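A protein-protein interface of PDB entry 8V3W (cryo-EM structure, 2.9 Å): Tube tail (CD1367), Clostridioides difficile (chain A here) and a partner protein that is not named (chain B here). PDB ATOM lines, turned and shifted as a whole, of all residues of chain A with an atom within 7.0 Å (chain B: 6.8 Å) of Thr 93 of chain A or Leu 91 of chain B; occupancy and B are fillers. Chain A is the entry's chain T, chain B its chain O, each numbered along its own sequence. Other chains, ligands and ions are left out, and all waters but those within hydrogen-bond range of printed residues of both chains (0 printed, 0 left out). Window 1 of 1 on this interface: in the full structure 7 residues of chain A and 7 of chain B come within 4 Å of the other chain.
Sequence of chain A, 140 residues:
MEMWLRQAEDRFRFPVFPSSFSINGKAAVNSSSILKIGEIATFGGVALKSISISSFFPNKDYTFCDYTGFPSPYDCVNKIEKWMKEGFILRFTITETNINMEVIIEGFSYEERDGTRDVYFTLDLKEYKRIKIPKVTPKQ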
ATOM      1  N   GLU A   2       3.853  23.300   6.125  1.00  0.00           N
ATOM      2  CA  GLU A   2       4.540  22.052   6.410  1.00  0.00           C
ATOM      3  C   GLU A   2       5.657  22.306   7.409  1.00  0.00           C
ATOM      4  O   GLU A   2       6.170  23.419   7.527  1.00  0.00           O
ATOM      5  CB  GLU A   2       5.117  21.415   5.141  1.00  0.00           C
ATOM      6  CG  GLU A   2       4.122  21.228   4.021  1.00  0.00           C
ATOM      7  CD  GLU A   2       4.789  21.038   2.676  1.00  0.00           C
ATOM      8  OE1 GLU A   2       6.029  20.931   2.637  1.00  0.00           O
ATOM      9  OE2 GLU A   2       4.071  20.976   1.659  1.00  0.00           O
ATOM     10  N   MET A   3       6.030  21.255   8.132  1.00  0.00           N
ATOM     11  CA  MET A   3       7.116  21.310   9.100  1.00  0.00           C
ATOM     12  C   MET A   3       8.129  20.221   8.785  1.00  0.00           C
ATOM     13  O   MET A   3       7.755  19.062   8.591  1.00  0.00           O
ATOM     14  CB  MET A   3       6.587  21.160  10.526  1.00  0.00           C
ATOM     15  CG  MET A   3       7.565  21.609  11.580  1.00  0.00           C
ATOM     16  SD  MET A   3       7.044  21.189  13.243  1.00  0.00           S
ATOM     17  CE  MET A   3       5.666  22.299  13.413  1.00  0.00           C
ATOM     18  N   TRP A   4       9.405  20.599   8.720  1.00  0.00           N
ATOM     19  CA  TRP A   4      10.484  19.701   8.332  1.00  0.00           C
ATOM     20  C   TRP A   4      11.636  19.798   9.321  1.00  0.00           C
ATOM     21  O   TRP A   4      11.966  20.886   9.794  1.00  0.00           O
ATOM     22  CB  TRP A   4      11.012  20.033   6.933  1.00  0.00           C
ATOM     23  CG  TRP A   4      10.038  19.860   5.815  1.00  0.00           C
ATOM     24  CD1 TRP A   4       9.051  20.718   5.454  1.00  0.00           C
ATOM     25  CD2 TRP A   4       9.985  18.775   4.886  1.00  0.00           C
ATOM     26  NE1 TRP A   4       8.372  20.232   4.366  1.00  0.00           N
ATOM     27  CE2 TRP A   4       8.929  19.037   3.999  1.00  0.00           C
ATOM     28  CE3 TRP A   4      10.724  17.602   4.724  1.00  0.00           C
ATOM     29  CZ2 TRP A   4       8.593  18.174   2.969  1.00  0.00           C
ATOM     30  CZ3 TRP A   4      10.389  16.750   3.703  1.00  0.00           C
ATOM     31  CH2 TRP A   4       9.333  17.038   2.837  1.00  0.00           C
ATOM     32  N   LEU A   5      12.257  18.658   9.611  1.00  0.00           N
ATOM     33  CA  LEU A   5      13.528  18.593  10.324  1.00  0.00           C
ATOM     34  C   LEU A   5      14.489  17.788   9.468  1.00  0.00           C
ATOM     35  O   LEU A   5      14.194  16.642   9.123  1.00  0.00           O
ATOM     36  CB  LEU A   5      13.372  17.943  11.702  1.00  0.00           C
ATOM     37  CG  LEU A   5      13.590  18.773  12.964  1.00  0.00           C
ATOM     38  CD1 LEU A   5      13.643  17.860  14.171  1.00  0.00           C
ATOM     39  CD2 LEU A   5      14.855  19.591  12.862  1.00  0.00           C
ATOM     40  N   ARG A   6      15.632  18.374   9.130  1.00  0.00           N
ATOM     41  CA  ARG A   6      16.559  17.769   8.183  1.00  0.00           C
ATOM     42  C   ARG A   6      17.957  17.727   8.774  1.00  0.00           C
ATOM     43  O   ARG A   6      18.424  18.715   9.347  1.00  0.00           O
ATOM     44  CB  ARG A   6      16.568  18.538   6.860  1.00  0.00           C
ATOM     45  CG  ARG A   6      15.201  18.632   6.212  1.00  0.00           C
ATOM     46  CD  ARG A   6      15.253  19.308   4.853  1.00  0.00           C
ATOM     47  NE  ARG A   6      15.118  20.754   4.945  1.00  0.00           N
ATOM     48  CZ  ARG A   6      15.910  21.619   4.326  1.00  0.00           C
ATOM     49  NH1 ARG A   6      16.899  21.215   3.549  1.00  0.00           N
ATOM     50  NH2 ARG A   6      15.699  22.920   4.492  1.00  0.00           N
ATOM     51  N   ARG A  11      15.902  13.659   5.718  1.00  0.00           N
ATOM     52  CA  ARG A  11      14.799  14.582   5.941  1.00  0.00           C
ATOM     53  C   ARG A  11      13.624  13.878   6.603  1.00  0.00           C
ATOM     54  O   ARG A  11      13.321  12.723   6.296  1.00  0.00           O
ATOM     55  CB  ARG A  11      14.342  15.226   4.631  1.00  0.00           C
ATOM     56  CG  ARG A  11      15.454  15.933   3.893  1.00  0.00           C
ATOM     57  CD  ARG A  11      15.502  15.565   2.432  1.00  0.00           C
ATOM     58  NE  ARG A  11      14.195  15.716   1.809  1.00  0.00           N
ATOM     59  CZ  ARG A  11      13.942  15.457   0.534  1.00  0.00           C
ATOM     60  NH1 ARG A  11      14.890  15.043  -0.290  1.00  0.00           N
ATOM     61  NH2 ARG A  11      12.707  15.626   0.071  1.00  0.00           N
ATOM     62  N   PHE A  14       6.793  16.142   9.548  1.00  0.00           N
ATOM     63  CA  PHE A  14       5.853  15.785  10.607  1.00  0.00           C
ATOM     64  C   PHE A  14       4.501  15.397  10.019  1.00  0.00           C
ATOM     65  O   PHE A  14       3.972  16.117   9.170  1.00  0.00           O
ATOM     66  CB  PHE A  14       5.688  16.934  11.596  1.00  0.00           C
ATOM     67  CG  PHE A  14       6.884  17.152  12.473  1.00  0.00           C
ATOM     68  CD1 PHE A  14       8.002  17.808  11.996  1.00  0.00           C
ATOM     69  CD2 PHE A  14       6.900  16.678  13.769  1.00  0.00           C
ATOM     70  CE1 PHE A  14       9.101  18.002  12.797  1.00  0.00           C
ATOM     71  CE2 PHE A  14       7.999  16.867  14.574  1.00  0.00           C
ATOM     72  CZ  PHE A  14       9.101  17.530  14.086  1.00  0.00           C
ATOM     73  N   PHE A  17       0.295  18.481  11.638  1.00  0.00           N
ATOM     74  CA  PHE A  17       0.707  19.847  11.925  1.00  0.00           C
ATOM     75  C   PHE A  17       0.128  20.300  13.265  1.00  0.00           C
ATOM     76  O   PHE A  17      -1.041  20.041  13.556  1.00  0.00           O
ATOM     77  CB  PHE A  17       0.251  20.784  10.812  1.00  0.00           C
ATOM     78  CG  PHE A  17       1.057  22.042  10.709  1.00  0.00           C
ATOM     79  CD1 PHE A  17       2.287  22.039  10.084  1.00  0.00           C
ATOM     80  CD2 PHE A  17       0.587  23.226  11.238  1.00  0.00           C
ATOM     81  CE1 PHE A  17       3.028  23.190   9.990  1.00  0.00           C
ATOM     82  CE2 PHE A  17       1.329  24.377  11.145  1.00  0.00           C
ATOM     83  CZ  PHE A  17       2.551  24.358  10.522  1.00  0.00           C
ATOM     84  N   ARG A  91      18.483  21.515  10.519  1.00  0.00           N
ATOM     85  CA  ARG A  91      17.803  22.654   9.921  1.00  0.00           C
ATOM     86  C   ARG A  91      16.300  22.492  10.093  1.00  0.00           C
ATOM     87  O   ARG A  91      15.732  21.471   9.697  1.00  0.00           O
ATOM     88  CB  ARG A  91      18.162  22.803   8.443  1.00  0.00           C
ATOM     89  CG  ARG A  91      17.618  24.067   7.800  1.00  0.00           C
ATOM     90  CD  ARG A  91      18.319  24.388   6.496  1.00  0.00           C
ATOM     91  NE  ARG A  91      19.707  24.782   6.703  1.00  0.00           N
ATOM     92  CZ  ARG A  91      20.090  26.000   7.059  1.00  0.00           C
ATOM     93  NH1 ARG A  91      19.218  26.982   7.205  1.00  0.00           N
ATOM     94  NH2 ARG A  91      21.378  26.237   7.271  1.00  0.00           N
ATOM     95  N   PHE A  92      15.664  23.505  10.674  1.00  0.00           N
ATOM     96  CA  PHE A  92      14.240  23.499  10.977  1.00  0.00           C
ATOM     97  C   PHE A  92      13.551  24.559  10.136  1.00  0.00           C
ATOM     98  O   PHE A  92      14.013  25.701  10.074  1.00  0.00           O
ATOM     99  CB  PHE A  92      14.006  23.767  12.463  1.00  0.00           C
ATOM    100  CG  PHE A  92      12.561  23.808  12.860  1.00  0.00           C
ATOM    101  CD1 PHE A  92      11.797  22.659  12.886  1.00  0.00           C
ATOM    102  CD2 PHE A  92      11.970  25.003  13.217  1.00  0.00           C
ATOM    103  CE1 PHE A  92      10.472  22.704  13.259  1.00  0.00           C
ATOM    104  CE2 PHE A  92      10.649  25.053  13.588  1.00  0.00           C
ATOM    105  CZ  PHE A  92       9.899  23.902  13.610  1.00  0.00           C
ATOM    106  N   THR A  93      12.449  24.188   9.496  1.00  0.00           N
ATOM    107  CA  THR A  93      11.755  25.101   8.604  1.00  0.00           C
ATOM    108  C   THR A  93      10.251  24.900   8.705  1.00  0.00           C
ATOM    109  O   THR A  93       9.774  23.775   8.858  1.00  0.00           O
ATOM    110  CB  THR A  93      12.224  24.919   7.153  1.00  0.00           C
ATOM    111  OG1 THR A  93      11.419  25.719   6.283  1.00  0.00           O
ATOM    112  CG2 THR A  93      12.129  23.477   6.739  1.00  0.00           C
ATOM    113  N   ILE A  94       9.514  26.006   8.656  1.00  0.00           N
ATOM    114  CA  ILE A  94       8.065  25.998   8.506  1.00  0.00           C
ATOM    115  C   ILE A  94       7.748  26.778   7.243  1.00  0.00           C
ATOM    116  O   ILE A  94       8.080  27.964   7.144  1.00  0.00           O
ATOM    117  CB  ILE A  94       7.354  26.613   9.721  1.00  0.00           C
ATOM    118  CG1 ILE A  94       7.665  25.821  10.987  1.00  0.00           C
ATOM    119  CG2 ILE A  94       5.858  26.654   9.491  1.00  0.00           C
ATOM    120  CD1 ILE A  94       7.068  26.421  12.231  1.00  0.00           C
ATOM    121  N   THR A  95       7.116  26.121   6.280  1.00  0.00           N
ATOM    122  CA  THR A  95       6.913  26.742   4.982  1.00  0.00           C
ATOM    123  C   THR A  95       5.880  27.859   5.077  1.00  0.00           C
ATOM    124  O   THR A  95       5.028  27.873   5.967  1.00  0.00           O
ATOM    125  CB  THR A  95       6.480  25.701   3.950  1.00  0.00           C
ATOM    126  OG1 THR A  95       5.185  25.196   4.282  1.00  0.00           O
ATOM    127  CG2 THR A  95       7.464  24.554   3.926  1.00  0.00           C
ATOM    128  N   GLU A  96       5.990  28.816   4.158  1.00  0.00           N
ATOM    129  CA  GLU A  96       5.119  29.984   4.067  1.00  0.00           C
ATOM    130  C   GLU A  96       5.282  30.948   5.235  1.00  0.00           C
ATOM    131  O   GLU A  96       4.403  31.776   5.473  1.00  0.00           O
ATOM    132  CB  GLU A  96       3.651  29.571   3.935  1.00  0.00           C
ATOM    133  CG  GLU A  96       3.232  29.226   2.531  1.00  0.00           C
ATOM    134  CD  GLU A  96       2.321  28.023   2.483  1.00  0.00           C
ATOM    135  OE1 GLU A  96       2.839  26.889   2.510  1.00  0.00           O
ATOM    136  OE2 GLU A  96       1.087  28.207   2.427  1.00  0.00           O
ATOM    137  N   THR A  97       6.386  30.864   5.973  1.00  0.00           N
ATOM    138  CA  THR A  97       6.694  31.803   7.048  1.00  0.00           C
ATOM    139  C   THR A  97       8.142  32.245   6.873  1.00  0.00           C
ATOM    140  O   THR A  97       8.756  32.019   5.829  1.00  0.00           O
ATOM    141  CB  THR A  97       6.466  31.187   8.437  1.00  0.00           C
ATOM    142  OG1 THR A  97       7.406  30.134   8.656  1.00  0.00           O
ATOM    143  CG2 THR A  97       5.061  30.635   8.572  1.00  0.00           C
ATOM    144  N   ILE A  99      10.511  31.257   9.149  1.00  0.00           N
ATOM    145  CA  ILE A  99      11.238  30.387  10.068  1.00  0.00           C
ATOM    146  C   ILE A  99      12.052  29.401   9.235  1.00  0.00           C
ATOM    147  O   ILE A  99      11.512  28.466   8.650  1.00  0.00           O
ATOM    148  CB  ILE A  99      10.293  29.671  11.033  1.00  0.00           C
ATOM    149  CG1 ILE A  99       9.465  30.693  11.815  1.00  0.00           C
ATOM    150  CG2 ILE A  99      11.075  28.794  11.982  1.00  0.00           C
ATOM    151  CD1 ILE A  99       8.150  30.169  12.315  1.00  0.00           C
ATOM    152  N   ASN A 100      13.366  29.626   9.173  1.00  0.00           N
ATOM    153  CA  ASN A 100      14.271  28.716   8.474  1.00  0.00           C
ATOM    154  C   ASN A 100      15.665  28.948   9.052  1.00  0.00           C
ATOM    155  O   ASN A 100      16.327  29.923   8.688  1.00  0.00           O
ATOM    156  CB  ASN A 100      14.233  28.959   6.976  1.00  0.00           C
ATOM    157  CG  ASN A 100      14.840  27.829   6.186  1.00  0.00           C
ATOM    158  OD1 ASN A 100      15.244  26.816   6.747  1.00  0.00           O
ATOM    159  ND2 ASN A 100      14.903  27.991   4.877  1.00  0.00           N
ATOM    160  N   MET A 101      16.101  28.059   9.940  1.00  0.00           N
ATOM    161  CA  MET A 101      17.346  28.277  10.665  1.00  0.00           C
ATOM    162  C   MET A 101      17.904  26.947  11.144  1.00  0.00           C
ATOM    163  O   MET A 101      17.246  25.908  11.072  1.00  0.00           O
ATOM    164  CB  MET A 101      17.132  29.221  11.848  1.00  0.00           C
ATOM    165  CG  MET A 101      16.230  28.647  12.913  1.00  0.00           C
ATOM    166  SD  MET A 101      15.787  29.835  14.183  1.00  0.00           S
ATOM    167  CE  MET A 101      14.394  29.012  14.934  1.00  0.00           C
ATOM    168  N   LEU B  82      17.214  22.571  -7.240  1.00  0.00           N
ATOM    169  CA  LEU B  82      15.768  22.716  -7.194  1.00  0.00           C
ATOM    170  C   LEU B  82      15.083  22.357  -8.504  1.00  0.00           C
ATOM    171  O   LEU B  82      13.860  22.196  -8.515  1.00  0.00           O
ATOM    172  CB  LEU B  82      15.400  24.150  -6.804  1.00  0.00           C
ATOM    173  CG  LEU B  82      15.966  24.669  -5.481  1.00  0.00           C
ATOM    174  CD1 LEU B  82      15.466  26.070  -5.206  1.00  0.00           C
ATOM    175  CD2 LEU B  82      15.606  23.743  -4.338  1.00  0.00           C
ATOM    176  N   TYR B  87      11.794  18.908  -4.335  1.00  0.00           N
ATOM    177  CA  TYR B  87      11.107  19.152  -3.076  1.00  0.00           C
ATOM    178  C   TYR B  87       9.699  19.646  -3.370  1.00  0.00           C
ATOM    179  O   TYR B  87       9.337  19.904  -4.519  1.00  0.00           O
ATOM    180  CB  TYR B  87      11.846  20.181  -2.213  1.00  0.00           C
ATOM    181  CG  TYR B  87      13.307  19.889  -1.984  1.00  0.00           C
ATOM    182  CD1 TYR B  87      13.708  18.845  -1.166  1.00  0.00           C
ATOM    183  CD2 TYR B  87      14.287  20.668  -2.576  1.00  0.00           C
ATOM    184  CE1 TYR B  87      15.043  18.580  -0.949  1.00  0.00           C
ATOM    185  CE2 TYR B  87      15.624  20.411  -2.366  1.00  0.00           C
ATOM    186  CZ  TYR B  87      15.997  19.369  -1.553  1.00  0.00           C
ATOM    187  OH  TYR B  87      17.330  19.113  -1.343  1.00  0.00           O
ATOM    188  N   THR B  88       8.898  19.777  -2.319  1.00  0.00           N
ATOM    189  CA  THR B  88       7.586  20.385  -2.459  1.00  0.00           C
ATOM    190  C   THR B  88       7.730  21.870  -2.796  1.00  0.00           C
ATOM    191  O   THR B  88       8.818  22.444  -2.738  1.00  0.00           O
ATOM    192  CB  THR B  88       6.770  20.198  -1.182  1.00  0.00           C
ATOM    193  OG1 THR B  88       7.227  21.117  -0.186  1.00  0.00           O
ATOM    194  CG2 THR B  88       6.917  18.784  -0.658  1.00  0.00           C
ATOM    195  N   LYS B  89       6.612  22.497  -3.159  1.00  0.00           N
ATOM    196  CA  LYS B  89       6.669  23.882  -3.615  1.00  0.00           C
ATOM    197  C   LYS B  89       7.124  24.828  -2.508  1.00  0.00           C
ATOM    198  O   LYS B  89       7.971  25.701  -2.738  1.00  0.00           O
ATOM    199  CB  LYS B  89       5.312  24.308  -4.164  1.00  0.00           C
ATOM    200  CG  LYS B  89       4.925  23.586  -5.433  1.00  0.00           C
ATOM    201  CD  LYS B  89       3.996  24.429  -6.284  1.00  0.00           C
ATOM    202  CE  LYS B  89       2.673  24.681  -5.587  1.00  0.00           C
ATOM    203  NZ  LYS B  89       1.639  25.206  -6.522  1.00  0.00           N
ATOM    204  N   GLY B  90       6.585  24.669  -1.300  1.00  0.00           N
ATOM    205  CA  GLY B  90       6.973  25.551  -0.212  1.00  0.00           C
ATOM    206  C   GLY B  90       8.430  25.396   0.175  1.00  0.00           C
ATOM    207  O   GLY B  90       9.131  26.387   0.420  1.00  0.00           O
ATOM    208  N   LEU B  91       8.907  24.152   0.243  1.00  0.00           N
ATOM    209  CA  LEU B  91      10.309  23.923   0.560  1.00  0.00           C
ATOM    210  C   LEU B  91      11.216  24.510  -0.512  1.00  0.00           C
ATOM    211  O   LEU B  91      12.253  25.105  -0.198  1.00  0.00           O
ATOM    212  CB  LEU B  91      10.572  22.429   0.741  1.00  0.00           C
ATOM    213  CG  LEU B  91      11.785  22.083   1.605  1.00  0.00           C
ATOM    214  CD1 LEU B  91      11.712  22.799   2.939  1.00  0.00           C
ATOM    215  CD2 LEU B  91      11.906  20.588   1.806  1.00  0.00           C
ATOM    216  N   THR B  92      10.838  24.368  -1.785  1.00  0.00           N
ATOM    217  CA  THR B  92      11.632  24.966  -2.855  1.00  0.00           C
ATOM    218  C   THR B  92      11.682  26.480  -2.724  1.00  0.00           C
ATOM    219  O   THR B  92      12.735  27.089  -2.926  1.00  0.00           O
ATOM    220  CB  THR B  92      11.080  24.578  -4.225  1.00  0.00           C
ATOM    221  OG1 THR B  92       9.682  24.872  -4.278  1.00  0.00           O
ATOM    222  CG2 THR B  92      11.301  23.107  -4.503  1.00  0.00           C
ATOM    223  N   GLU B  93      10.558  27.106  -2.377  1.00  0.00           N
ATOM    224  CA  GLU B  93      10.544  28.557  -2.217  1.00  0.00           C
ATOM    225  C   GLU B  93      11.471  29.006  -1.089  1.00  0.00           C
ATOM    226  O   GLU B  93      12.292  29.924  -1.261  1.00  0.00           O
ATOM    227  CB  GLU B  93       9.116  29.022  -1.960  1.00  0.00           C
ATOM    228  CG  GLU B  93       8.901  30.495  -2.166  1.00  0.00           C
ATOM    229  CD  GLU B  93       7.624  30.982  -1.521  1.00  0.00           C
ATOM    230  OE1 GLU B  93       6.598  30.283  -1.641  1.00  0.00           O
ATOM    231  OE2 GLU B  93       7.644  32.065  -0.902  1.00  0.00           O
ATOM    232  N   SER B  94      11.357  28.363   0.077  1.00  0.00           N
ATOM    233  CA  SER B  94      12.211  28.733   1.203  1.00  0.00           C
ATOM    234  C   SER B  94      13.683  28.533   0.869  1.00  0.00           C
ATOM    235  O   SER B  94      14.525  29.395   1.166  1.00  0.00           O
ATOM    236  CB  SER B  94      11.834  27.922   2.439  1.00  0.00           C
ATOM    237  OG  SER B  94      10.475  28.107   2.783  1.00  0.00           O
ATOM    238  N   GLU B  95      14.013  27.402   0.242  1.00  0.00           N
ATOM    239  CA  GLU B  95      15.402  27.123  -0.082  1.00  0.00           C
ATOM    240  C   GLU B  95      15.941  28.096  -1.118  1.00  0.00           C
ATOM    241  O   GLU B  95      17.105  28.492  -1.048  1.00  0.00           O
ATOM    242  CB  GLU B  95      15.549  25.681  -0.556  1.00  0.00           C
ATOM    243  CG  GLU B  95      15.359  24.661   0.552  1.00  0.00           C
ATOM    244  CD  GLU B  95      16.337  24.853   1.694  1.00  0.00           C
ATOM    245  OE1 GLU B  95      17.453  24.300   1.621  1.00  0.00           O
ATOM    246  OE2 GLU B  95      15.995  25.552   2.668  1.00  0.00           O
ATOM    247  N   ALA B  96      15.119  28.493  -2.092  1.00  0.00           N
ATOM    248  CA  ALA B  96      15.572  29.477  -3.069  1.00  0.00           C
ATOM    249  C   ALA B  96      15.900  30.802  -2.400  1.00  0.00           C
ATOM    250  O   ALA B  96      16.941  31.414  -2.685  1.00  0.00           O
ATOM    251  CB  ALA B  96      14.510  29.671  -4.148  1.00  0.00           C
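The side-chain carboxylate (OE1) of Glu 2 of chain A is in hydrogen-bond range of the side-chain hydroxyl (OG1) of Thr 88 of chain B (3.1 Å).
OE2 of Glu 95 of chain B lies within salt-bridge range of NH2 of Arg 6 of chain A, 3.2 Å away.
The side-chain amide nitrogen of Asn 100 of chain A is in hydrogen-bond range of the side-chain carboxylate of Glu 95 of chain B (3.5 Å).
The backbone NH (N) of Glu 2 of chain A lies within hydrogen-bond range of the side-chain hydroxyl (OG1) of Thr 95 of chain A, at 3.0 Å.
The backbone NH (N) of Trp 4 of chain A sits at hydrogen-bond distance from the backbone carbonyl oxygen (O) of Thr 93 of chain A (3.2 Å).
The side-chain hydroxyl (OG1) of Thr 95 of chain A lies within hydrogen-bond range of the side-chain carboxylate (OE1) of Glu 96 of chain A, at 3.4 Å.
OG1 of Thr 88 of chain B sits at hydrogen-bond distance from N of Leu 91 of chain B (3.5 Å).
OG1 of Thr 92 of chain B sits at hydrogen-bond distance from O of Thr 88 of chain B, 3.0 Å away.
O of Gly 90 of chain B lies within hydrogen-bond range of OG of Ser 94 of chain B (3.2 Å).
Among the printed residues, pairs that only touch across the chains: Arg 11 of chain A with Tyr 87 of chain B, Thr 93 of chain A with Leu 91 of chain B, Asn 100 of chain A with Ser 94 of chain B, Thr 95 of chain A with Gly 90 of chain B and Thr 95 of chain A with Leu 91 of chain B.
Thr 93 of chain A touches just one residue of chain B: Leu 91 (3.9 Å).
Of the printed residues of chain A, Thr 88 of chain B touches Glu 2 (3.1 Å).
Of chain A, only Thr 95 comes within 4 Å of Gly 90 of chain B.
Of the printed residues of chain A, Leu 91 of chain B touches Thr 93 and Thr 95.
Of the printed residues of chain A, Glu 95 of chain B touches Arg 6 (3.2 Å) and Asn 100 (3.5 Å).
The nearest printed residue of chain A that does not touch Leu 91 of chain B is Trp 4 of chain A (4.01 Å).
The nearest printed residue of chain B that does not touch Glu 2 of chain A is Leu 91 of chain B (4.9 Å).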
